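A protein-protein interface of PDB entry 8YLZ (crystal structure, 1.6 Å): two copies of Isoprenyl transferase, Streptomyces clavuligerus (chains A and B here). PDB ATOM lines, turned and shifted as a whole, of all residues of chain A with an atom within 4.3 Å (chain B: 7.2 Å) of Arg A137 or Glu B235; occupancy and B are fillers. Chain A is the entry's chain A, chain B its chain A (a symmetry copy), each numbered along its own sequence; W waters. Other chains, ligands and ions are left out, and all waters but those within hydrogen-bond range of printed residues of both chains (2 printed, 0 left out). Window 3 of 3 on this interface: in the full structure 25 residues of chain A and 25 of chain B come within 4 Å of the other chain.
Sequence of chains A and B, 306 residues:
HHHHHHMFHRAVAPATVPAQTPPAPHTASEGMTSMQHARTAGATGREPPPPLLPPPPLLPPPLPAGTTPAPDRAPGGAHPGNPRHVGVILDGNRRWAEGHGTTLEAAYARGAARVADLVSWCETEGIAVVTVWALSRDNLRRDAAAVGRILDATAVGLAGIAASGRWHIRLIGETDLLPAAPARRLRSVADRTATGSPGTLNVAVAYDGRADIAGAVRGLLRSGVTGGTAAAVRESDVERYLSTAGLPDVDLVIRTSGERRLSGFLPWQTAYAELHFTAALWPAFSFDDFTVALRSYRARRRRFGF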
ATOM      1  N   LEU A 135      -9.144  13.507  20.946  1.00  0.00           N
ATOM      2  CA  LEU A 135      -9.879  12.597  20.071  1.00  0.00           C
ATOM      3  C   LEU A 135     -10.221  13.284  18.761  1.00  0.00           C
ATOM      4  O   LEU A 135     -10.879  14.326  18.771  1.00  0.00           O
ATOM      5  CB  LEU A 135     -11.174  12.131  20.745  1.00  0.00           C
ATOM      6  CG  LEU A 135     -11.412  10.658  21.017  1.00  0.00           C
ATOM      7  CD1 LEU A 135     -12.866  10.490  21.443  1.00  0.00           C
ATOM      8  CD2 LEU A 135     -11.106   9.841  19.785  1.00  0.00           C
ATOM      9  N   SER A 136      -9.824  12.683  17.641  1.00  0.00           N
ATOM     10  CA  SER A 136     -10.235  13.220  16.356  1.00  0.00           C
ATOM     11  C   SER A 136     -11.593  12.674  15.954  1.00  0.00           C
ATOM     12  O   SER A 136     -12.080  11.687  16.491  1.00  0.00           O
ATOM     13  CB  SER A 136      -9.222  12.891  15.264  1.00  0.00           C
ATOM     14  OG  SER A 136      -9.231  11.508  15.018  1.00  0.00           O
ATOM     15  N   ARG A 137     -12.217  13.362  15.007  1.00  0.00           N
ATOM     16  CA  ARG A 137     -13.425  12.833  14.389  1.00  0.00           C
ATOM     17  C   ARG A 137     -13.122  11.575  13.591  1.00  0.00           C
ATOM     18  O   ARG A 137     -13.899  10.612  13.610  1.00  0.00           O
ATOM     19  CB  ARG A 137     -14.032  13.894  13.484  1.00  0.00           C
ATOM     20  CG  ARG A 137     -15.337  13.513  12.838  1.00  0.00           C
ATOM     21  CD  ARG A 137     -15.904  14.732  12.134  1.00  0.00           C
ATOM     22  NE  ARG A 137     -15.178  14.939  10.887  1.00  0.00           N
ATOM     23  CZ  ARG A 137     -15.473  15.873   9.993  1.00  0.00           C
ATOM     24  NH1 ARG A 137     -16.513  16.674  10.148  1.00  0.00           N
ATOM     25  NH2 ARG A 137     -14.697  16.012   8.927  1.00  0.00           N
ATOM     26  N   ASP A 138     -11.998  11.577  12.869  1.00  0.00           N
ATOM     27  CA  ASP A 138     -11.621  10.406  12.086  1.00  0.00           C
ATOM     28  C   ASP A 138     -11.472   9.178  12.975  1.00  0.00           C
ATOM     29  O   ASP A 138     -11.827   8.064  12.574  1.00  0.00           O
ATOM     30  CB  ASP A 138     -10.331  10.686  11.317  1.00  0.00           C
ATOM     31  CG  ASP A 138     -10.573  11.491  10.056  1.00  0.00           C
ATOM     32  OD1 ASP A 138     -11.718  11.956   9.861  1.00  0.00           O
ATOM     33  OD2 ASP A 138      -9.623  11.660   9.258  1.00  0.00           O
ATOM     34  N   ASN A 139     -10.975   9.361  14.194  1.00  0.00           N
ATOM     35  CA  ASN A 139     -10.781   8.247  15.108  1.00  0.00           C
ATOM     36  C   ASN A 139     -12.030   7.917  15.919  1.00  0.00           C
ATOM     37  O   ASN A 139     -11.943   7.141  16.876  1.00  0.00           O
ATOM     38  CB  ASN A 139      -9.606   8.521  16.050  1.00  0.00           C
ATOM     39  CG  ASN A 139      -8.253   8.237  15.398  1.00  0.00           C
ATOM     40  OD1 ASN A 139      -8.058   7.189  14.775  1.00  0.00           O
ATOM     41  ND2 ASN A 139      -7.307   9.167  15.555  1.00  0.00           N
ATOM     42  N   LEU A 140     -13.184   8.489  15.569  1.00  0.00           N
ATOM     43  CA  LEU A 140     -14.442   7.960  16.084  1.00  0.00           C
ATOM     44  C   LEU A 140     -14.825   6.653  15.411  1.00  0.00           C
ATOM     45  O   LEU A 140     -15.745   5.974  15.882  1.00  0.00           O
ATOM     46  CB  LEU A 140     -15.571   8.978  15.908  1.00  0.00           C
ATOM     47  CG  LEU A 140     -15.414  10.320  16.617  1.00  0.00           C
ATOM     48  CD1 LEU A 140     -16.553  11.256  16.239  1.00  0.00           C
ATOM     49  CD2 LEU A 140     -15.364  10.115  18.123  1.00  0.00           C
ATOM     50  N   GLU A 174     -16.955  18.634  17.801  1.00  0.00           N
ATOM     51  CA  GLU A 174     -18.360  18.350  17.521  1.00  0.00           C
ATOM     52  C   GLU A 174     -18.823  17.297  18.527  1.00  0.00           C
ATOM     53  O   GLU A 174     -18.923  16.105  18.233  1.00  0.00           O
ATOM     54  CB  GLU A 174     -18.531  17.899  16.073  1.00  0.00           C
ATOM     55  CG  GLU A 174     -17.907  18.848  15.023  1.00  0.00           C
ATOM     56  CD  GLU A 174     -17.092  18.112  13.948  1.00  0.00           C
ATOM     57  OE1 GLU A 174     -17.714  17.619  12.973  1.00  0.00           O
ATOM     58  OE2 GLU A 174     -15.845  17.993  14.075  1.00  0.00           O
ATOM     59  N   LEU A 177     -21.438  14.520  18.156  1.00  0.00           N
ATOM     60  CA  LEU A 177     -21.107  13.252  17.514  1.00  0.00           C
ATOM     61  C   LEU A 177     -20.779  12.120  18.483  1.00  0.00           C
ATOM     62  O   LEU A 177     -20.668  10.969  18.043  1.00  0.00           O
ATOM     63  CB  LEU A 177     -19.907  13.433  16.572  1.00  0.00           C
ATOM     64  CG  LEU A 177     -20.032  14.406  15.397  1.00  0.00           C
ATOM     65  CD1 LEU A 177     -18.729  14.398  14.589  1.00  0.00           C
ATOM     66  CD2 LEU A 177     -21.249  14.083  14.520  1.00  0.00           C
ATOM     67  N   ALA A 206     -13.737  14.730  19.244  1.00  0.00           N
ATOM     68  CA  ALA A 206     -14.443  14.725  17.960  1.00  0.00           C
ATOM     69  C   ALA A 206     -14.171  16.007  17.171  1.00  0.00           C
ATOM     70  O   ALA A 206     -15.066  16.592  16.556  1.00  0.00           O
ATOM     71  CB  ALA A 206     -15.957  14.523  18.154  1.00  0.00           C
ATOM     72  N   TYR A 207     -12.921  16.474  17.217  1.00  0.00           N
ATOM     73  CA  TYR A 207     -12.517  17.700  16.536  1.00  0.00           C
ATOM     74  C   TYR A 207     -11.885  17.364  15.196  1.00  0.00           C
ATOM     75  O   TYR A 207     -11.204  16.350  15.068  1.00  0.00           O
ATOM     76  CB  TYR A 207     -11.508  18.498  17.379  1.00  0.00           C
ATOM     77  CG  TYR A 207     -10.981  19.692  16.644  1.00  0.00           C
ATOM     78  CD1 TYR A 207     -11.692  20.876  16.617  1.00  0.00           C
ATOM     79  CD2 TYR A 207      -9.799  19.608  15.909  1.00  0.00           C
ATOM     80  CE1 TYR A 207     -11.237  21.958  15.917  1.00  0.00           C
ATOM     81  CE2 TYR A 207      -9.352  20.662  15.187  1.00  0.00           C
ATOM     82  CZ  TYR A 207     -10.061  21.845  15.205  1.00  0.00           C
ATOM     83  OH  TYR A 207      -9.579  22.905  14.467  1.00  0.00           O
ATOM     84  N   ASP A 208     -12.125  18.227  14.211  1.00  0.00           N
ATOM     85  CA  ASP A 208     -11.529  18.150  12.883  1.00  0.00           C
ATOM     86  C   ASP A 208     -11.291  19.563  12.364  1.00  0.00           C
ATOM     87  O   ASP A 208     -12.193  20.401  12.436  1.00  0.00           O
ATOM     88  CB  ASP A 208     -12.464  17.398  11.936  1.00  0.00           C
ATOM     89  CG  ASP A 208     -11.816  17.108  10.598  1.00  0.00           C
ATOM     90  OD1 ASP A 208     -12.052  17.927   9.697  1.00  0.00           O
ATOM     91  OD2 ASP A 208     -11.150  16.048  10.425  1.00  0.00           O
ATOM     92  N   ARG A 210     -10.793  20.707   9.211  1.00  0.00           N
ATOM     93  CA  ARG A 210     -11.586  21.097   8.054  1.00  0.00           C
ATOM     94  C   ARG A 210     -13.038  21.351   8.449  1.00  0.00           C
ATOM     95  O   ARG A 210     -13.672  22.278   7.927  1.00  0.00           O
ATOM     96  CB  ARG A 210     -11.443  20.026   6.956  1.00  0.00           C
ATOM     97  CG  ARG A 210     -10.067  20.064   6.253  1.00  0.00           C
ATOM     98  CD  ARG A 210      -9.907  18.942   5.217  1.00  0.00           C
ATOM     99  NE  ARG A 210      -8.621  18.988   4.532  1.00  0.00           N
ATOM    100  CZ  ARG A 210      -8.332  18.210   3.496  1.00  0.00           C
ATOM    101  NH1 ARG A 210      -9.183  17.286   3.071  1.00  0.00           N
ATOM    102  NH2 ARG A 210      -7.157  18.348   2.882  1.00  0.00           N
ATOM    103  N   ALA A 211     -13.564  20.598   9.426  1.00  0.00           N
ATOM    104  CA  ALA A 211     -14.899  20.886   9.950  1.00  0.00           C
ATOM    105  C   ALA A 211     -14.935  22.219  10.688  1.00  0.00           C
ATOM    106  O   ALA A 211     -15.931  22.952  10.622  1.00  0.00           O
ATOM    107  CB  ALA A 211     -15.351  19.764  10.874  1.00  0.00           C
ATOM    108  N   ALA A 214     -15.094  24.766   7.981  1.00  0.00           N
ATOM    109  CA  ALA A 214     -16.434  24.724   7.399  1.00  0.00           C
ATOM    110  C   ALA A 214     -17.484  25.350   8.313  1.00  0.00           C
ATOM    111  O   ALA A 214     -18.451  25.942   7.823  1.00  0.00           O
ATOM    112  CB  ALA A 214     -16.812  23.283   7.066  1.00  0.00           C
ATOM    113  N   VAL B 233     -23.802  23.500   3.097  1.00  0.00           N
ATOM    114  CA  VAL B 233     -22.386  23.578   2.720  1.00  0.00           C
ATOM    115  C   VAL B 233     -21.576  22.457   3.374  1.00  0.00           C
ATOM    116  O   VAL B 233     -21.607  22.263   4.591  1.00  0.00           O
ATOM    117  CB  VAL B 233     -21.797  24.964   3.052  1.00  0.00           C
ATOM    118  CG1 VAL B 233     -21.997  25.291   4.518  1.00  0.00           C
ATOM    119  CG2 VAL B 233     -20.313  25.018   2.697  1.00  0.00           C
ATOM    120  N   ARG B 234     -20.874  21.708   2.531  1.00  0.00           N
ATOM    121  CA  ARG B 234     -20.044  20.580   2.918  1.00  0.00           C
ATOM    122  C   ARG B 234     -18.581  21.008   2.925  1.00  0.00           C
ATOM    123  O   ARG B 234     -18.213  22.043   2.359  1.00  0.00           O
ATOM    124  CB  ARG B 234     -20.237  19.412   1.947  1.00  0.00           C
ATOM    125  CG  ARG B 234     -21.654  18.820   1.871  1.00  0.00           C
ATOM    126  CD  ARG B 234     -22.120  18.198   3.187  1.00  0.00           C
ATOM    127  NE  ARG B 234     -22.847  19.136   4.036  1.00  0.00           N
ATOM    128  CZ  ARG B 234     -24.147  19.061   4.293  1.00  0.00           C
ATOM    129  NH1 ARG B 234     -24.898  18.100   3.779  1.00  0.00           N
ATOM    130  NH2 ARG B 234     -24.706  19.975   5.082  1.00  0.00           N
ATOM    131  N   GLU B 235     -17.750  20.209   3.601  1.00  0.00           N
ATOM    132  CA  GLU B 235     -16.315  20.471   3.568  1.00  0.00           C
ATOM    133  C   GLU B 235     -15.796  20.429   2.135  1.00  0.00           C
ATOM    134  O   GLU B 235     -14.953  21.249   1.743  1.00  0.00           O
ATOM    135  CB  GLU B 235     -15.579  19.475   4.470  1.00  0.00           C
ATOM    136  CG  GLU B 235     -15.767  19.777   5.970  1.00  0.00           C
ATOM    137  CD  GLU B 235     -15.640  18.552   6.875  1.00  0.00           C
ATOM    138  OE1 GLU B 235     -14.819  17.661   6.576  1.00  0.00           O
ATOM    139  OE2 GLU B 235     -16.340  18.505   7.909  1.00  0.00           O
ATOM    140  N   SER B 236     -16.321  19.512   1.320  1.00  0.00           N
ATOM    141  CA  SER B 236     -15.875  19.459  -0.068  1.00  0.00           C
ATOM    142  C   SER B 236     -16.269  20.703  -0.852  1.00  0.00           C
ATOM    143  O   SER B 236     -15.602  21.032  -1.844  1.00  0.00           O
ATOM    144  CB  SER B 236     -16.410  18.193  -0.746  1.00  0.00           C
ATOM    145  OG  SER B 236     -17.821  18.108  -0.616  1.00  0.00           O
ATOM    146  N   ASP B 237     -17.313  21.421  -0.434  1.00  0.00           N
ATOM    147  CA  ASP B 237     -17.648  22.676  -1.094  1.00  0.00           C
ATOM    148  C   ASP B 237     -16.708  23.805  -0.703  1.00  0.00           C
ATOM    149  O   ASP B 237     -16.432  24.689  -1.522  1.00  0.00           O
ATOM    150  CB  ASP B 237     -19.093  23.083  -0.796  1.00  0.00           C
ATOM    151  CG  ASP B 237     -20.098  22.059  -1.272  1.00  0.00           C
ATOM    152  OD1 ASP B 237     -19.984  21.606  -2.436  1.00  0.00           O
ATOM    153  OD2 ASP B 237     -21.003  21.707  -0.477  1.00  0.00           O
ATOM    154  N   VAL B 238     -16.197  23.804   0.530  1.00  0.00           N
ATOM    155  CA  VAL B 238     -15.187  24.794   0.893  1.00  0.00           C
ATOM    156  C   VAL B 238     -13.925  24.570   0.068  1.00  0.00           C
ATOM    157  O   VAL B 238     -13.349  25.505  -0.505  1.00  0.00           O
ATOM    158  CB  VAL B 238     -14.900  24.732   2.405  1.00  0.00           C
ATOM    159  CG1 VAL B 238     -13.733  25.634   2.755  1.00  0.00           C
ATOM    160  CG2 VAL B 238     -16.169  25.116   3.199  1.00  0.00           C
ATOM    161  N   GLU B 239     -13.505  23.307  -0.027  1.00  0.00           N
ATOM    162  CA  GLU B 239     -12.302  22.960  -0.773  1.00  0.00           C
ATOM    163  C   GLU B 239     -12.387  23.425  -2.225  1.00  0.00           C
ATOM    164  O   GLU B 239     -11.417  23.958  -2.771  1.00  0.00           O
ATOM    165  CB  GLU B 239     -12.099  21.451  -0.723  1.00  0.00           C
ATOM    166  CG  GLU B 239     -10.844  20.981  -1.489  1.00  0.00           C
ATOM    167  CD  GLU B 239     -10.572  19.484  -1.327  1.00  0.00           C
ATOM    168  OE1 GLU B 239     -10.352  19.015  -0.184  1.00  0.00           O
ATOM    169  OE2 GLU B 239     -10.570  18.758  -2.359  1.00  0.00           O
ATOM    170  N   ARG B 240     -13.555  23.239  -2.855  1.00  0.00           N
ATOM    171  CA  ARG B 240     -13.763  23.550  -4.264  1.00  0.00           C
ATOM    172  C   ARG B 240     -13.647  25.029  -4.548  1.00  0.00           C
ATOM    173  O   ARG B 240     -13.386  25.419  -5.688  1.00  0.00           O
ATOM    174  CB  ARG B 240     -15.167  23.093  -4.688  1.00  0.00           C
ATOM    175  CG  ARG B 240     -15.326  21.641  -5.051  1.00  0.00           C
ATOM    176  CD  ARG B 240     -16.776  21.175  -4.774  1.00  0.00           C
ATOM    177  NE  ARG B 240     -17.774  22.194  -5.084  1.00  0.00           N
ATOM    178  CZ  ARG B 240     -18.104  22.575  -6.313  1.00  0.00           C
ATOM    179  NH1 ARG B 240     -17.588  21.988  -7.385  1.00  0.00           N
ATOM    180  NH2 ARG B 240     -18.974  23.565  -6.474  1.00  0.00           N
ATOM    181  N   TYR B 241     -13.859  25.873  -3.539  1.00  0.00           N
ATOM    182  CA  TYR B 241     -13.846  27.309  -3.726  1.00  0.00           C
ATOM    183  C   TYR B 241     -12.615  27.977  -3.143  1.00  0.00           C
ATOM    184  O   TYR B 241     -12.487  29.203  -3.238  1.00  0.00           O
ATOM    185  CB  TYR B 241     -15.121  27.927  -3.139  1.00  0.00           C
ATOM    186  CG  TYR B 241     -16.272  27.741  -4.101  1.00  0.00           C
ATOM    187  CD1 TYR B 241     -17.238  26.769  -3.892  1.00  0.00           C
ATOM    188  CD2 TYR B 241     -16.315  28.482  -5.276  1.00  0.00           C
ATOM    189  CE1 TYR B 241     -18.283  26.581  -4.814  1.00  0.00           C
ATOM    190  CE2 TYR B 241     -17.337  28.303  -6.210  1.00  0.00           C
ATOM    191  CZ  TYR B 241     -18.320  27.357  -5.966  1.00  0.00           C
ATOM    192  OH  TYR B 241     -19.336  27.179  -6.883  1.00  0.00           O
ATOM    193  N   TRP B 268      -5.440  24.091   3.947  1.00  0.00           N
ATOM    194  CA  TRP B 268      -6.350  22.993   3.647  1.00  0.00           C
ATOM    195  C   TRP B 268      -5.590  21.775   3.148  1.00  0.00           C
ATOM    196  O   TRP B 268      -5.737  20.678   3.687  1.00  0.00           O
ATOM    197  CB  TRP B 268      -7.397  23.444   2.628  1.00  0.00           C
ATOM    198  CG  TRP B 268      -8.556  22.486   2.491  1.00  0.00           C
ATOM    199  CD1 TRP B 268      -8.627  21.380   1.677  1.00  0.00           C
ATOM    200  CD2 TRP B 268      -9.815  22.551   3.189  1.00  0.00           C
ATOM    201  NE1 TRP B 268      -9.844  20.744   1.848  1.00  0.00           N
ATOM    202  CE2 TRP B 268     -10.594  21.456   2.753  1.00  0.00           C
ATOM    203  CE3 TRP B 268     -10.350  23.423   4.145  1.00  0.00           C
ATOM    204  CZ2 TRP B 268     -11.889  21.222   3.229  1.00  0.00           C
ATOM    205  CZ3 TRP B 268     -11.648  23.186   4.624  1.00  0.00           C
ATOM    206  CH2 TRP B 268     -12.396  22.094   4.160  1.00  0.00           C
ATOM    207  N   TYR B 272      -2.733  17.009   6.332  1.00  0.00           N
ATOM    208  CA  TYR B 272      -2.182  15.696   6.646  1.00  0.00           C
ATOM    209  C   TYR B 272      -0.813  15.468   6.026  1.00  0.00           C
ATOM    210  O   TYR B 272      -0.361  14.327   5.903  1.00  0.00           O
ATOM    211  CB  TYR B 272      -3.165  14.608   6.211  1.00  0.00           C
ATOM    212  CG  TYR B 272      -4.452  14.687   6.994  1.00  0.00           C
ATOM    213  CD1 TYR B 272      -4.583  14.048   8.219  1.00  0.00           C
ATOM    214  CD2 TYR B 272      -5.529  15.419   6.515  1.00  0.00           C
ATOM    215  CE1 TYR B 272      -5.767  14.120   8.939  1.00  0.00           C
ATOM    216  CE2 TYR B 272      -6.711  15.505   7.233  1.00  0.00           C
ATOM    217  CZ  TYR B 272      -6.817  14.855   8.445  1.00  0.00           C
ATOM    218  OH  TYR B 272      -7.989  14.933   9.170  1.00  0.00           O
HETATM  219  O   HOH W   1      -8.326  17.489  11.461  1.00  0.00           O
HETATM  220  O   HOH W   2     -10.199  16.215   7.700  1.00  0.00           O
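NH2 of Arg A137 lies within salt-bridge range of OE1 of Glu B235, 2.9 Å away.
The guanidinium group (NH1) of Arg A210 lies within salt-bridge range of the side-chain carboxylate (OE1) of Glu B239.
NH2 of Arg A210 sits at hydrogen-bond distance from O of Trp B268 (2.8 Å).
OE1 of Glu A174 is in salt-bridge range of NH1 of Arg A137 (3.2 Å).
The backbone NH (N) of Arg A137 is in hydrogen-bond range of the backbone carbonyl oxygen (O) of Tyr A207, at 3.2 Å.
The side-chain carboxylate (OD1) of Asp A208 is in salt-bridge range of the guanidinium group (NH2) of Arg A137.
The backbone NH of Arg A210 sits at hydrogen-bond distance from the side-chain carboxylate of Asp A208, at 3.1 Å.
OD1 of Asp A208 lies within hydrogen-bond range of N of Ala A211 (3.1 Å).
The side-chain carboxylate (OE1) of Glu B239 lies within hydrogen-bond range of the indole nitrogen (NE1) of Trp B268, at 2.7 Å.
Tyr B272 touches Asp A138.
Asp A208 touches Tyr B272.
CG of Glu B235 touches O of Arg A210, 3.8 Å away.
Glu B235 touches Ala A211 (OE2 to CB, 3.4 Å).
CB of Ala A214 touches CG of Glu B235, at 3.8 Å.
Of the printed residues of chain B, Arg A137 touches Glu B235 (2.9 Å).
Of the printed residues of chain B, Asp A138 touches Tyr B272 (3.7 Å).
Leu A140 touches none of the printed residues of chain B.
Of the printed residues of chain B, Ala A211 touches Glu B235.
Glu B235 touches four residues of chain A.
Of the printed residues of chain A, Tyr B272 touches Asp A138 (3.7 Å) and Asp A208 (3.6 Å).
The nearest residue of chain B that does not touch Arg A137 is Tyr B272 (6.8 Å).
The nearest residue of chain A that does not touch Glu B235 is Asp A208 (4.2 Å).
Hydrophobic or aromatic side chains of chain B that line the printed part of chain A: Trp B268 and Tyr B272.
Hydrophobic or aromatic side chains of chain A that line the printed part of chain B: Ala A211 and Ala A214.
No position is printed for both chains.
Water W2 bridges OD2 of Asp A208 and OH of Tyr B272.
Water W1 lies within hydrogen-bond range of the side-chain carboxylate of Asp A208 (3.3 Å) and the side-chain hydroxyl of Tyr B272 (3.4 Å).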
